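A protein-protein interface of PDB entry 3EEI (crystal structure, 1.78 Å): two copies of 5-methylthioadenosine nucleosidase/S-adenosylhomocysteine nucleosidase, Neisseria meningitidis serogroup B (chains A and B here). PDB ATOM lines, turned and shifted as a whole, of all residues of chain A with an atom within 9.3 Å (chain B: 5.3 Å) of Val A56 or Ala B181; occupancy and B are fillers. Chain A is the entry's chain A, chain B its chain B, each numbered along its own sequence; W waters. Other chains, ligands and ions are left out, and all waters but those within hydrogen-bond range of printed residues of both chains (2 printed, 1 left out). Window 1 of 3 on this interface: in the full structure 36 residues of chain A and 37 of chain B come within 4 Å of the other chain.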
ATOM      1  N   ILE A   9      17.237 -15.135 -17.787  1.00  0.00           N
ATOM      2  CA  ILE A   9      15.982 -15.424 -18.508  1.00  0.00           C
ATOM      3  C   ILE A   9      16.317 -16.169 -19.794  1.00  0.00           C
ATOM      4  O   ILE A   9      17.111 -15.656 -20.585  1.00  0.00           O
ATOM      5  CB  ILE A   9      15.298 -14.111 -18.971  1.00  0.00           C
ATOM      6  CG1 ILE A   9      15.219 -13.056 -17.839  1.00  0.00           C
ATOM      7  CG2 ILE A   9      13.908 -14.398 -19.531  1.00  0.00           C
ATOM      8  CD1 ILE A   9      14.256 -13.454 -16.722  1.00  0.00           C
ATOM      9  N   PHE A  34       3.872 -18.847 -15.978  1.00  0.00           N
ATOM     10  CA  PHE A  34       5.349 -18.747 -15.984  1.00  0.00           C
ATOM     11  C   PHE A  34       6.014 -19.477 -14.824  1.00  0.00           C
ATOM     12  O   PHE A  34       5.493 -19.471 -13.711  1.00  0.00           O
ATOM     13  CB  PHE A  34       5.778 -17.288 -15.898  1.00  0.00           C
ATOM     14  CG  PHE A  34       5.304 -16.468 -17.056  1.00  0.00           C
ATOM     15  CD1 PHE A  34       6.040 -16.422 -18.226  1.00  0.00           C
ATOM     16  CD2 PHE A  34       4.105 -15.794 -16.999  1.00  0.00           C
ATOM     17  CE1 PHE A  34       5.594 -15.689 -19.326  1.00  0.00           C
ATOM     18  CE2 PHE A  34       3.656 -15.039 -18.090  1.00  0.00           C
ATOM     19  CZ  PHE A  34       4.396 -14.991 -19.254  1.00  0.00           C
ATOM     20  N   SER A  51      10.977 -18.132 -19.981  1.00  0.00           N
ATOM     21  CA  SER A  51       9.965 -17.122 -20.384  1.00  0.00           C
ATOM     22  C   SER A  51       8.934 -17.626 -21.351  1.00  0.00           C
ATOM     23  O   SER A  51       7.787 -17.145 -21.381  1.00  0.00           O
ATOM     24  CB  SER A  51      10.667 -15.902 -20.962  1.00  0.00           C
ATOM     25  OG  SER A  51      11.371 -16.211 -22.161  1.00  0.00           O
ATOM     26  N   GLY A  52       9.319 -18.603 -22.169  1.00  0.00           N
ATOM     27  CA  GLY A  52       8.555 -18.873 -23.361  1.00  0.00           C
ATOM     28  C   GLY A  52       9.060 -17.963 -24.488  1.00  0.00           C
ATOM     29  O   GLY A  52       9.844 -17.023 -24.247  1.00  0.00           O
ATOM     30  N   ILE A  53       8.591 -18.226 -25.702  1.00  0.00           N
ATOM     31  CA  ILE A  53       9.114 -17.592 -26.914  1.00  0.00           C
ATOM     32  C   ILE A  53       8.449 -16.259 -27.234  1.00  0.00           C
ATOM     33  O   ILE A  53       7.232 -16.130 -27.064  1.00  0.00           O
ATOM     34  CB  ILE A  53       8.974 -18.575 -28.097  1.00  0.00           C
ATOM     35  CG1 ILE A  53       9.993 -19.721 -27.866  1.00  0.00           C
ATOM     36  CG2 ILE A  53       9.151 -17.869 -29.449  1.00  0.00           C
ATOM     37  CD1 ILE A  53       9.638 -21.031 -28.595  1.00  0.00           C
ATOM     38  N   GLY A  54       9.255 -15.269 -27.655  1.00  0.00           N
ATOM     39  CA  GLY A  54       8.730 -14.026 -28.240  1.00  0.00           C
ATOM     40  C   GLY A  54       8.631 -12.900 -27.252  1.00  0.00           C
ATOM     41  O   GLY A  54       8.903 -13.075 -26.049  1.00  0.00           O
ATOM     42  N   LYS A  55       8.233 -11.730 -27.760  1.00  0.00           N
ATOM     43  CA  LYS A  55       8.455 -10.525 -27.002  1.00  0.00           C
ATOM     44  C   LYS A  55       7.555 -10.398 -25.773  1.00  0.00           C
ATOM     45  O   LYS A  55       7.994  -9.919 -24.709  1.00  0.00           O
ATOM     46  CB  LYS A  55       8.212  -9.329 -27.892  1.00  0.00           C
ATOM     47  CG  LYS A  55       9.216  -9.124 -28.993  1.00  0.00           C
ATOM     48  CD  LYS A  55       8.844  -7.711 -29.528  1.00  0.00           C
ATOM     49  CE  LYS A  55       8.753  -7.612 -30.980  1.00  0.00           C
ATOM     50  NZ  LYS A  55       8.887  -6.147 -31.316  1.00  0.00           N
ATOM     51  N   VAL A  56       6.276 -10.749 -25.926  1.00  0.00           N
ATOM     52  CA  VAL A  56       5.350 -10.590 -24.792  1.00  0.00           C
ATOM     53  C   VAL A  56       5.759 -11.544 -23.640  1.00  0.00           C
ATOM     54  O   VAL A  56       5.822 -11.153 -22.484  1.00  0.00           O
ATOM     55  CB  VAL A  56       3.879 -10.834 -25.226  1.00  0.00           C
ATOM     56  CG1 VAL A  56       2.943 -11.021 -23.975  1.00  0.00           C
ATOM     57  CG2 VAL A  56       3.418  -9.710 -26.159  1.00  0.00           C
ATOM     58  N   ASN A  57       5.993 -12.818 -23.968  1.00  0.00           N
ATOM     59  CA  ASN A  57       6.420 -13.776 -22.982  1.00  0.00           C
ATOM     60  C   ASN A  57       7.695 -13.299 -22.269  1.00  0.00           C
ATOM     61  O   ASN A  57       7.812 -13.360 -21.030  1.00  0.00           O
ATOM     62  CB  ASN A  57       6.692 -15.154 -23.672  1.00  0.00           C
ATOM     63  CG  ASN A  57       5.407 -15.974 -23.942  1.00  0.00           C
ATOM     64  OD1 ASN A  57       5.394 -16.879 -24.823  1.00  0.00           O
ATOM     65  ND2 ASN A  57       4.363 -15.720 -23.184  1.00  0.00           N
ATOM     66  N   ALA A  58       8.690 -12.840 -23.025  1.00  0.00           N
ATOM     67  CA  ALA A  58       9.948 -12.452 -22.374  1.00  0.00           C
ATOM     68  C   ALA A  58       9.730 -11.226 -21.497  1.00  0.00           C
ATOM     69  O   ALA A  58      10.285 -11.140 -20.404  1.00  0.00           O
ATOM     70  CB  ALA A  58      11.015 -12.193 -23.412  1.00  0.00           C
ATOM     71  N   ALA A  59       8.885 -10.310 -21.960  1.00  0.00           N
ATOM     72  CA  ALA A  59       8.668  -9.060 -21.212  1.00  0.00           C
ATOM     73  C   ALA A  59       8.011  -9.365 -19.860  1.00  0.00           C
ATOM     74  O   ALA A  59       8.413  -8.839 -18.821  1.00  0.00           O
ATOM     75  CB  ALA A  59       7.775  -8.100 -22.008  1.00  0.00           C
ATOM     76  N   VAL A  60       6.979 -10.186 -19.897  1.00  0.00           N
ATOM     77  CA  VAL A  60       6.215 -10.482 -18.684  1.00  0.00           C
ATOM     78  C   VAL A  60       7.102 -11.258 -17.709  1.00  0.00           C
ATOM     79  O   VAL A  60       7.148 -10.976 -16.508  1.00  0.00           O
ATOM     80  CB  VAL A  60       4.970 -11.289 -19.016  1.00  0.00           C
ATOM     81  CG1 VAL A  60       4.277 -11.793 -17.727  1.00  0.00           C
ATOM     82  CG2 VAL A  60       3.983 -10.451 -19.825  1.00  0.00           C
ATOM     83  N   ALA A  61       7.839 -12.238 -18.226  1.00  0.00           N
ATOM     84  CA  ALA A  61       8.702 -13.025 -17.348  1.00  0.00           C
ATOM     85  C   ALA A  61       9.747 -12.151 -16.682  1.00  0.00           C
ATOM     86  O   ALA A  61      10.015 -12.273 -15.494  1.00  0.00           O
ATOM     87  CB  ALA A  61       9.362 -14.146 -18.157  1.00  0.00           C
ATOM     88  N   THR A  62      10.359 -11.263 -17.453  1.00  0.00           N
ATOM     89  CA  THR A  62      11.362 -10.357 -16.945  1.00  0.00           C
ATOM     90  C   THR A  62      10.778  -9.400 -15.903  1.00  0.00           C
ATOM     91  O   THR A  62      11.436  -9.097 -14.902  1.00  0.00           O
ATOM     92  CB  THR A  62      11.971  -9.527 -18.085  1.00  0.00           C
ATOM     93  OG1 THR A  62      12.586 -10.411 -19.026  1.00  0.00           O
ATOM     94  CG2 THR A  62      13.063  -8.582 -17.569  1.00  0.00           C
ATOM     95  N   ALA A  63       9.572  -8.899 -16.165  1.00  0.00           N
ATOM     96  CA  ALA A  63       8.973  -7.925 -15.232  1.00  0.00           C
ATOM     97  C   ALA A  63       8.665  -8.653 -13.919  1.00  0.00           C
ATOM     98  O   ALA A  63       8.890  -8.133 -12.817  1.00  0.00           O
ATOM     99  CB  ALA A  63       7.693  -7.366 -15.826  1.00  0.00           C
ATOM    100  N   TRP A  64       8.154  -9.876 -14.053  1.00  0.00           N
ATOM    101  CA  TRP A  64       7.894 -10.704 -12.886  1.00  0.00           C
ATOM    102  C   TRP A  64       9.128 -10.922 -12.028  1.00  0.00           C
ATOM    103  O   TRP A  64       9.087 -10.686 -10.817  1.00  0.00           O
ATOM    104  CB  TRP A  64       7.308 -12.022 -13.312  1.00  0.00           C
ATOM    105  CG  TRP A  64       7.239 -13.021 -12.222  1.00  0.00           C
ATOM    106  CD1 TRP A  64       6.834 -12.817 -10.940  1.00  0.00           C
ATOM    107  CD2 TRP A  64       7.564 -14.417 -12.333  1.00  0.00           C
ATOM    108  NE1 TRP A  64       6.890 -14.017 -10.233  1.00  0.00           N
ATOM    109  CE2 TRP A  64       7.344 -15.003 -11.065  1.00  0.00           C
ATOM    110  CE3 TRP A  64       8.012 -15.223 -13.386  1.00  0.00           C
ATOM    111  CZ2 TRP A  64       7.569 -16.343 -10.819  1.00  0.00           C
ATOM    112  CZ3 TRP A  64       8.236 -16.577 -13.133  1.00  0.00           C
ATOM    113  CH2 TRP A  64       8.019 -17.109 -11.859  1.00  0.00           C
ATOM    114  N   HIS A 100      14.636  -3.623 -31.380  1.00  0.00           N
ATOM    115  CA  HIS A 100      13.549  -4.314 -32.122  1.00  0.00           C
ATOM    116  C   HIS A 100      13.706  -4.114 -33.623  1.00  0.00           C
ATOM    117  O   HIS A 100      13.672  -2.964 -34.109  1.00  0.00           O
ATOM    118  CB  HIS A 100      12.188  -3.730 -31.736  1.00  0.00           C
ATOM    119  CG  HIS A 100      11.858  -3.887 -30.277  1.00  0.00           C
ATOM    120  ND1 HIS A 100      11.350  -5.056 -29.748  1.00  0.00           N
ATOM    121  CD2 HIS A 100      11.950  -3.009 -29.245  1.00  0.00           C
ATOM    122  CE1 HIS A 100      11.140  -4.888 -28.449  1.00  0.00           C
ATOM    123  NE2 HIS A 100      11.505  -3.652 -28.119  1.00  0.00           N
ATOM    124  N   GLY A 152      12.713  -9.609 -32.961  1.00  0.00           N
ATOM    125  CA  GLY A 152      11.354  -9.369 -33.346  1.00  0.00           C
ATOM    126  C   GLY A 152      10.515 -10.629 -33.210  1.00  0.00           C
ATOM    127  O   GLY A 152      11.022 -11.683 -32.827  1.00  0.00           O
ATOM    128  N   ASP A 153       9.222 -10.508 -33.499  1.00  0.00           N
ATOM    129  CA  ASP A 153       8.281 -11.580 -33.141  1.00  0.00           C
ATOM    130  C   ASP A 153       8.163 -12.568 -34.297  1.00  0.00           C
ATOM    131  O   ASP A 153       7.090 -13.097 -34.609  1.00  0.00           O
ATOM    132  CB  ASP A 153       6.932 -11.026 -32.673  1.00  0.00           C
ATOM    133  CG  ASP A 153       6.716 -11.193 -31.186  1.00  0.00           C
ATOM    134  OD1 ASP A 153       5.698 -10.681 -30.680  1.00  0.00           O
ATOM    135  OD2 ASP A 153       7.550 -11.862 -30.528  1.00  0.00           O
ATOM    136  N   MET A 177      14.303 -13.454 -30.779  1.00  0.00           N
ATOM    137  CA  MET A 177      12.895 -13.053 -30.590  1.00  0.00           C
ATOM    138  C   MET A 177      12.595 -12.536 -29.184  1.00  0.00           C
ATOM    139  O   MET A 177      11.434 -12.207 -28.905  1.00  0.00           O
ATOM    140  CB  MET A 177      11.966 -14.250 -30.877  1.00  0.00           C
ATOM    141  CG  MET A 177      12.113 -14.735 -32.292  1.00  0.00           C
ATOM    142  SD  MET A 177      11.091 -16.196 -32.720  1.00  0.00           S
ATOM    143  CE  MET A 177       9.470 -15.700 -32.245  1.00  0.00           C
ATOM    144  N   GLU A 178      13.605 -12.479 -28.315  1.00  0.00           N
ATOM    145  CA  GLU A 178      13.354 -11.965 -26.934  1.00  0.00           C
ATOM    146  C   GLU A 178      14.224 -10.832 -26.430  1.00  0.00           C
ATOM    147  O   GLU A 178      13.787 -10.039 -25.553  1.00  0.00           O
ATOM    148  CB  GLU A 178      13.467 -13.115 -25.939  1.00  0.00           C
ATOM    149  CG  GLU A 178      12.429 -14.210 -26.208  1.00  0.00           C
ATOM    150  CD  GLU A 178      12.958 -15.312 -27.096  1.00  0.00           C
ATOM    151  OE1 GLU A 178      14.188 -15.535 -27.076  1.00  0.00           O
ATOM    152  OE2 GLU A 178      12.140 -15.965 -27.774  1.00  0.00           O
ATOM    153  N   ALA A 179      15.443 -10.730 -26.949  1.00  0.00           N
ATOM    154  CA  ALA A 179      16.426  -9.865 -26.339  1.00  0.00           C
ATOM    155  C   ALA A 179      15.936  -8.443 -26.213  1.00  0.00           C
ATOM    156  O   ALA A 179      16.154  -7.766 -25.185  1.00  0.00           O
ATOM    157  CB  ALA A 179      17.670  -9.862 -27.191  1.00  0.00           C
ATOM    158  N   ALA A 180      15.385  -7.918 -27.302  1.00  0.00           N
ATOM    159  CA  ALA A 180      14.960  -6.477 -27.241  1.00  0.00           C
ATOM    160  C   ALA A 180      13.796  -6.282 -26.271  1.00  0.00           C
ATOM    161  O   ALA A 180      13.635  -5.193 -25.677  1.00  0.00           O
ATOM    162  CB  ALA A 180      14.600  -5.949 -28.633  1.00  0.00           C
ATOM    163  N   ALA A 181      12.963  -7.304 -26.090  1.00  0.00           N
ATOM    164  CA  ALA A 181      11.854  -7.190 -25.102  1.00  0.00           C
ATOM    165  C   ALA A 181      12.394  -7.182 -23.671  1.00  0.00           C
ATOM    166  O   ALA A 181      11.902  -6.476 -22.785  1.00  0.00           O
ATOM    167  CB  ALA A 181      10.855  -8.332 -25.283  1.00  0.00           C
ATOM    168  N   ILE A 182      13.367  -8.044 -23.410  1.00  0.00           N
ATOM    169  CA  ILE A 182      13.997  -8.055 -22.108  1.00  0.00           C
ATOM    170  C   ILE A 182      14.703  -6.746 -21.863  1.00  0.00           C
ATOM    171  O   ILE A 182      14.571  -6.165 -20.786  1.00  0.00           O
ATOM    172  CB  ILE A 182      15.031  -9.216 -22.072  1.00  0.00           C
ATOM    173  CG1 ILE A 182      14.273 -10.514 -22.162  1.00  0.00           C
ATOM    174  CG2 ILE A 182      15.927  -9.142 -20.830  1.00  0.00           C
ATOM    175  CD1 ILE A 182      15.195 -11.786 -22.310  1.00  0.00           C
ATOM    176  N   GLN A 184      14.156  -3.766 -23.272  1.00  0.00           N
ATOM    177  CA  GLN A 184      13.200  -2.666 -23.097  1.00  0.00           C
ATOM    178  C   GLN A 184      12.544  -2.757 -21.718  1.00  0.00           C
ATOM    179  O   GLN A 184      12.290  -1.737 -21.066  1.00  0.00           O
ATOM    180  CB  GLN A 184      12.142  -2.720 -24.174  1.00  0.00           C
ATOM    181  CG  GLN A 184      11.005  -1.756 -23.927  1.00  0.00           C
ATOM    182  CD  GLN A 184       9.940  -1.794 -25.021  1.00  0.00           C
ATOM    183  OE1 GLN A 184      10.127  -2.415 -26.058  1.00  0.00           O
ATOM    184  NE2 GLN A 184       8.806  -1.143 -24.775  1.00  0.00           N
ATOM    185  N   THR A 185      12.241  -3.967 -21.271  1.00  0.00           N
ATOM    186  CA  THR A 185      11.669  -4.124 -19.930  1.00  0.00           C
ATOM    187  C   THR A 185      12.668  -3.655 -18.864  1.00  0.00           C
ATOM    188  O   THR A 185      12.317  -2.910 -17.940  1.00  0.00           O
ATOM    189  CB  THR A 185      11.276  -5.590 -19.701  1.00  0.00           C
ATOM    190  OG1 THR A 185      10.308  -5.962 -20.717  1.00  0.00           O
ATOM    191  CG2 THR A 185      10.645  -5.784 -18.277  1.00  0.00           C
ATOM    192  N   GLY B  54       2.859  -0.033 -27.646  1.00  0.00           N
ATOM    193  CA  GLY B  54       3.505  -1.239 -28.199  1.00  0.00           C
ATOM    194  C   GLY B  54       3.395  -2.460 -27.303  1.00  0.00           C
ATOM    195  O   GLY B  54       2.928  -2.356 -26.184  1.00  0.00           O
ATOM    196  N   LYS B  55       3.887  -3.610 -27.773  1.00  0.00           N
ATOM    197  CA  LYS B  55       3.561  -4.881 -27.113  1.00  0.00           C
ATOM    198  C   LYS B  55       4.265  -5.055 -25.792  1.00  0.00           C
ATOM    199  O   LYS B  55       3.673  -5.543 -24.835  1.00  0.00           O
ATOM    200  CB  LYS B  55       3.967  -6.052 -27.980  1.00  0.00           C
ATOM    201  CG  LYS B  55       3.323  -6.093 -29.346  1.00  0.00           C
ATOM    202  CD  LYS B  55       3.785  -7.507 -29.935  1.00  0.00           C
ATOM    203  CE  LYS B  55       3.662  -7.614 -31.356  1.00  0.00           C
ATOM    204  NZ  LYS B  55       3.712  -9.058 -31.686  1.00  0.00           N
ATOM    205  N   VAL B  56       5.568  -4.763 -25.770  1.00  0.00           N
ATOM    206  CA  VAL B  56       6.340  -4.872 -24.533  1.00  0.00           C
ATOM    207  C   VAL B  56       5.779  -3.972 -23.468  1.00  0.00           C
ATOM    208  O   VAL B  56       5.516  -4.397 -22.339  1.00  0.00           O
ATOM    209  CB  VAL B  56       7.836  -4.628 -24.745  1.00  0.00           C
ATOM    210  CG1 VAL B  56       8.567  -4.542 -23.390  1.00  0.00           C
ATOM    211  CG2 VAL B  56       8.407  -5.747 -25.644  1.00  0.00           C
ATOM    212  N   ALA B  58       2.762  -2.632 -23.182  1.00  0.00           N
ATOM    213  CA  ALA B  58       1.455  -3.108 -22.742  1.00  0.00           C
ATOM    214  C   ALA B  58       1.575  -4.383 -21.888  1.00  0.00           C
ATOM    215  O   ALA B  58       0.867  -4.538 -20.903  1.00  0.00           O
ATOM    216  CB  ALA B  58       0.534  -3.342 -23.959  1.00  0.00           C
ATOM    217  N   ALA B  59       2.419  -5.319 -22.297  1.00  0.00           N
ATOM    218  CA  ALA B  59       2.502  -6.562 -21.570  1.00  0.00           C
ATOM    219  C   ALA B  59       3.042  -6.336 -20.152  1.00  0.00           C
ATOM    220  O   ALA B  59       2.534  -6.922 -19.192  1.00  0.00           O
ATOM    221  CB  ALA B  59       3.364  -7.572 -22.342  1.00  0.00           C
ATOM    222  N   HIS B 100      -2.025 -11.557 -32.709  1.00  0.00           N
ATOM    223  CA  HIS B 100      -0.911 -10.767 -33.220  1.00  0.00           C
ATOM    224  C   HIS B 100      -0.857 -10.891 -34.742  1.00  0.00           C
ATOM    225  O   HIS B 100      -0.701 -11.980 -35.275  1.00  0.00           O
ATOM    226  CB  HIS B 100       0.428 -11.324 -32.729  1.00  0.00           C
ATOM    227  CG  HIS B 100       0.597 -11.343 -31.249  1.00  0.00           C
ATOM    228  ND1 HIS B 100       1.095 -10.260 -30.541  1.00  0.00           N
ATOM    229  CD2 HIS B 100       0.403 -12.335 -30.344  1.00  0.00           C
ATOM    230  CE1 HIS B 100       1.194 -10.594 -29.260  1.00  0.00           C
ATOM    231  NE2 HIS B 100       0.767 -11.842 -29.116  1.00  0.00           N
ATOM    232  N   SER B 151      -3.021  -6.955 -33.511  1.00  0.00           N
ATOM    233  CA  SER B 151      -2.021  -6.025 -33.003  1.00  0.00           C
ATOM    234  C   SER B 151      -0.626  -6.431 -33.485  1.00  0.00           C
ATOM    235  O   SER B 151      -0.324  -7.594 -33.716  1.00  0.00           O
ATOM    236  CB  SER B 151      -1.943  -6.090 -31.471  1.00  0.00           C
ATOM    237  OG  SER B 151      -3.228  -6.022 -30.872  1.00  0.00           O
ATOM    238  N   GLU B 178      -1.399  -2.798 -29.028  1.00  0.00           N
ATOM    239  CA  GLU B 178      -1.319  -3.337 -27.641  1.00  0.00           C
ATOM    240  C   GLU B 178      -2.220  -4.545 -27.338  1.00  0.00           C
ATOM    241  O   GLU B 178      -1.878  -5.354 -26.472  1.00  0.00           O
ATOM    242  CB  GLU B 178      -1.553  -2.250 -26.583  1.00  0.00           C
ATOM    243  CG  GLU B 178      -0.514  -1.086 -26.554  1.00  0.00           C
ATOM    244  CD  GLU B 178      -0.862  -0.015 -27.554  1.00  0.00           C
ATOM    245  OE1 GLU B 178      -2.078   0.120 -27.837  1.00  0.00           O
ATOM    246  OE2 GLU B 178       0.057   0.669 -28.054  1.00  0.00           O
ATOM    247  N   ALA B 179      -3.363  -4.655 -28.002  1.00  0.00           N
ATOM    248  CA  ALA B 179      -4.431  -5.540 -27.531  1.00  0.00           C
ATOM    249  C   ALA B 179      -3.980  -6.990 -27.455  1.00  0.00           C
ATOM    250  O   ALA B 179      -4.277  -7.679 -26.475  1.00  0.00           O
ATOM    251  CB  ALA B 179      -5.668  -5.395 -28.426  1.00  0.00           C
ATOM    252  N   ALA B 180      -3.255  -7.463 -28.449  1.00  0.00           N
ATOM    253  CA  ALA B 180      -2.837  -8.888 -28.365  1.00  0.00           C
ATOM    254  C   ALA B 180      -1.800  -9.128 -27.290  1.00  0.00           C
ATOM    255  O   ALA B 180      -1.705 -10.219 -26.720  1.00  0.00           O
ATOM    256  CB  ALA B 180      -2.356  -9.392 -29.684  1.00  0.00           C
ATOM    257  N   ALA B 181      -1.023  -8.093 -26.965  1.00  0.00           N
ATOM    258  CA  ALA B 181      -0.078  -8.253 -25.876  1.00  0.00           C
ATOM    259  C   ALA B 181      -0.843  -8.339 -24.549  1.00  0.00           C
ATOM    260  O   ALA B 181      -0.528  -9.149 -23.694  1.00  0.00           O
ATOM    261  CB  ALA B 181       0.867  -7.097 -25.865  1.00  0.00           C
ATOM    262  N   ILE B 182      -1.850  -7.484 -24.383  1.00  0.00           N
ATOM    263  CA  ILE B 182      -2.680  -7.531 -23.178  1.00  0.00           C
ATOM    264  C   ILE B 182      -3.403  -8.880 -23.100  1.00  0.00           C
ATOM    265  O   ILE B 182      -3.373  -9.553 -22.073  1.00  0.00           O
ATOM    266  CB  ILE B 182      -3.670  -6.355 -23.197  1.00  0.00           C
ATOM    267  CG1 ILE B 182      -2.877  -5.028 -23.149  1.00  0.00           C
ATOM    268  CG2 ILE B 182      -4.745  -6.512 -22.071  1.00  0.00           C
ATOM    269  CD1 ILE B 182      -3.777  -3.752 -23.335  1.00  0.00           C
ATOM    270  N   ALA B 183      -4.022  -9.283 -24.189  1.00  0.00           N
ATOM    271  CA  ALA B 183      -4.665 -10.588 -24.285  1.00  0.00           C
ATOM    272  C   ALA B 183      -3.747 -11.745 -23.951  1.00  0.00           C
ATOM    273  O   ALA B 183      -4.133 -12.667 -23.185  1.00  0.00           O
ATOM    274  CB  ALA B 183      -5.234 -10.787 -25.697  1.00  0.00           C
ATOM    275  N   GLN B 184      -2.562 -11.780 -24.560  1.00  0.00           N
ATOM    276  CA  GLN B 184      -1.642 -12.895 -24.292  1.00  0.00           C
ATOM    277  C   GLN B 184      -1.258 -12.880 -22.815  1.00  0.00           C
ATOM    278  O   GLN B 184      -1.079 -13.944 -22.198  1.00  0.00           O
ATOM    279  CB  GLN B 184      -0.366 -12.771 -25.148  1.00  0.00           C
ATOM    280  CG  GLN B 184       0.668 -13.866 -24.927  1.00  0.00           C
ATOM    281  CD  GLN B 184       1.893 -13.695 -25.805  1.00  0.00           C
ATOM    282  OE1 GLN B 184       1.846 -12.964 -26.814  1.00  0.00           O
ATOM    283  NE2 GLN B 184       3.006 -14.381 -25.447  1.00  0.00           N
ATOM    284  N   THR B 185      -1.094 -11.692 -22.256  1.00  0.00           N
ATOM    285  CA  THR B 185      -0.593 -11.590 -20.877  1.00  0.00           C
ATOM    286  C   THR B 185      -1.696 -12.097 -19.947  1.00  0.00           C
ATOM    287  O   THR B 185      -1.466 -12.851 -18.988  1.00  0.00           O
ATOM    288  CB  THR B 185      -0.207 -10.132 -20.517  1.00  0.00           C
ATOM    289  OG1 THR B 185       0.930  -9.709 -21.300  1.00  0.00           O
ATOM    290  CG2 THR B 185       0.150 -10.013 -19.019  1.00  0.00           C
ATOM    291  N   CYS B 186      -2.925 -11.703 -20.257  1.00  0.00           N
ATOM    292  CA  CYS B 186      -4.048 -12.158 -19.450  1.00  0.00           C
ATOM    293  C   CYS B 186      -4.193 -13.670 -19.570  1.00  0.00           C
ATOM    294  O   CYS B 186      -4.502 -14.345 -18.593  1.00  0.00           O
ATOM    295  CB  CYS B 186      -5.322 -11.435 -19.873  1.00  0.00           C
ATOM    296  SG  CYS B 186      -5.276  -9.700 -19.301  1.00  0.00           S
HETATM  297  O   HOH W   1       6.289  -7.516 -32.886  1.00  0.00           O
HETATM  298  O   HOH W   2       6.440  -1.437 -26.292  1.00  0.00           O
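Of the 16 printed residues of chain B, 7 touch a printed residue of chain A. Of the 27 printed residues of chain A, 8 touch a printed residue of chain B. Printed residues of chain A that touch a printed residue of chain B: Val A56, Asn A57, Ala A59, Val A60, Asp A153, Ala A181, Gln A184 and Thr A185.
Water W2 lies within hydrogen-bond range of NE2 of Gln A184 (2.8 Å) and N of Val B56 (3.5 Å). Water W1 lies within hydrogen-bond range of the side-chain amino group (NZ) of Lys B55 and the side-chain amino group (NZ) of Lys A55.
Val A56 touches Ala B59, and with the chains exchanged Ala A59 touches Val B56. Val A56 touches His B100, but with the chains exchanged His A100 does not touch Val B56 (4.01 Å). Val A56 touches Ala B181, and with the chains exchanged Ala A181 touches Val B56. Val A56 touches Thr B185, and with the chains exchanged Thr A185 touches Val B56. 13 positions are printed for both chains. Of the 13 pairs that touch across the chains among the printed residues, 8 have their exchanged pair printed and touching as well.
OD1 of Asn A57 sits close to O of Ile A53, at 3.0 Å. The backbone NH (N) of Lys A55 lies within hydrogen-bond range of the side-chain carboxylate (OD2) of Asp A153, 2.9 Å away. The side-chain amide oxygen (OE1) of Gln A184 lies within hydrogen-bond range of a ring nitrogen (NE2) of His A100, at 2.8 Å. NZ of Lys B55 sits at hydrogen-bond distance from ND1 of His B100 (3.1 Å). NE2 of His B100 sits at hydrogen-bond distance from OE1 of Gln B184, 2.8 Å away. OG1 of Thr B185 lies within hydrogen-bond range of O of Ala B181 (2.9 Å).
Val A56 touches just these residues of chain B: Ala B59 (3.8 Å), His B100 (3.9 Å), Ala B181 (3.7 Å), Gln B184 (3.3 Å) and Thr B185 (3.6 Å). Ala B181 touches just one residue of chain A: Val A56. No residue of chain A comes within 4 Å of Ala B183. Printed residues of chain A within 4 Å of Lys B55: Asp A153 (2.8 Å). Of the printed residues of chain A, Val B56 touches Ala A59, Ala A181, Gln A184 and Thr A185. Printed residues of chain B within 4 Å of Thr A185: Val B56. Of the printed residues of chain B, Ala A181 touches Val B56. Printed residues of chain B within 4 Å of Ala A59: Val B56. Ile B182 touches none of the printed residues of chain A. Ala A58 touches none of the printed residues of chain B. The nearest residue of chain B that does not touch Val A56 is Lys B55 (4.1 Å). The nearest residue of chain A that does not touch Ala B181 is Val A60 (6.1 Å). The nearest printed residue of chain B that does not touch Ala A59 is Ala B59 (4.5 Å).
The side-chain amide nitrogen (ND2) of Asn A57 lies close to the side-chain amide nitrogen (NE2) of Gln B184 (3.0 Å). The side-chain amino group (NZ) of Lys B55 lies within salt-bridge range of the side-chain carboxylate (OD1) of Asp A153 (2.8 Å).
Among the printed residues, merely in contact across the chains: Val A56 with Gln B184 (3.3 Å), Gln A184 with Val B56 (3.4 Å), Val A60 with Thr B185 (3.5 Å), Thr A185 with Val B56 (3.5 Å), Ala A181 with Val B56 (3.6 Å), Val A56 with Thr B185 (3.6 Å), Val A56 with Ala B181 (3.7 Å), Val A56 with Ala B59 (3.8 Å), Val A60 with Ala B59 (3.9 Å), Ala A59 with Val B56 (3.9 Å) and Val A56 with His B100 (3.9 Å).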
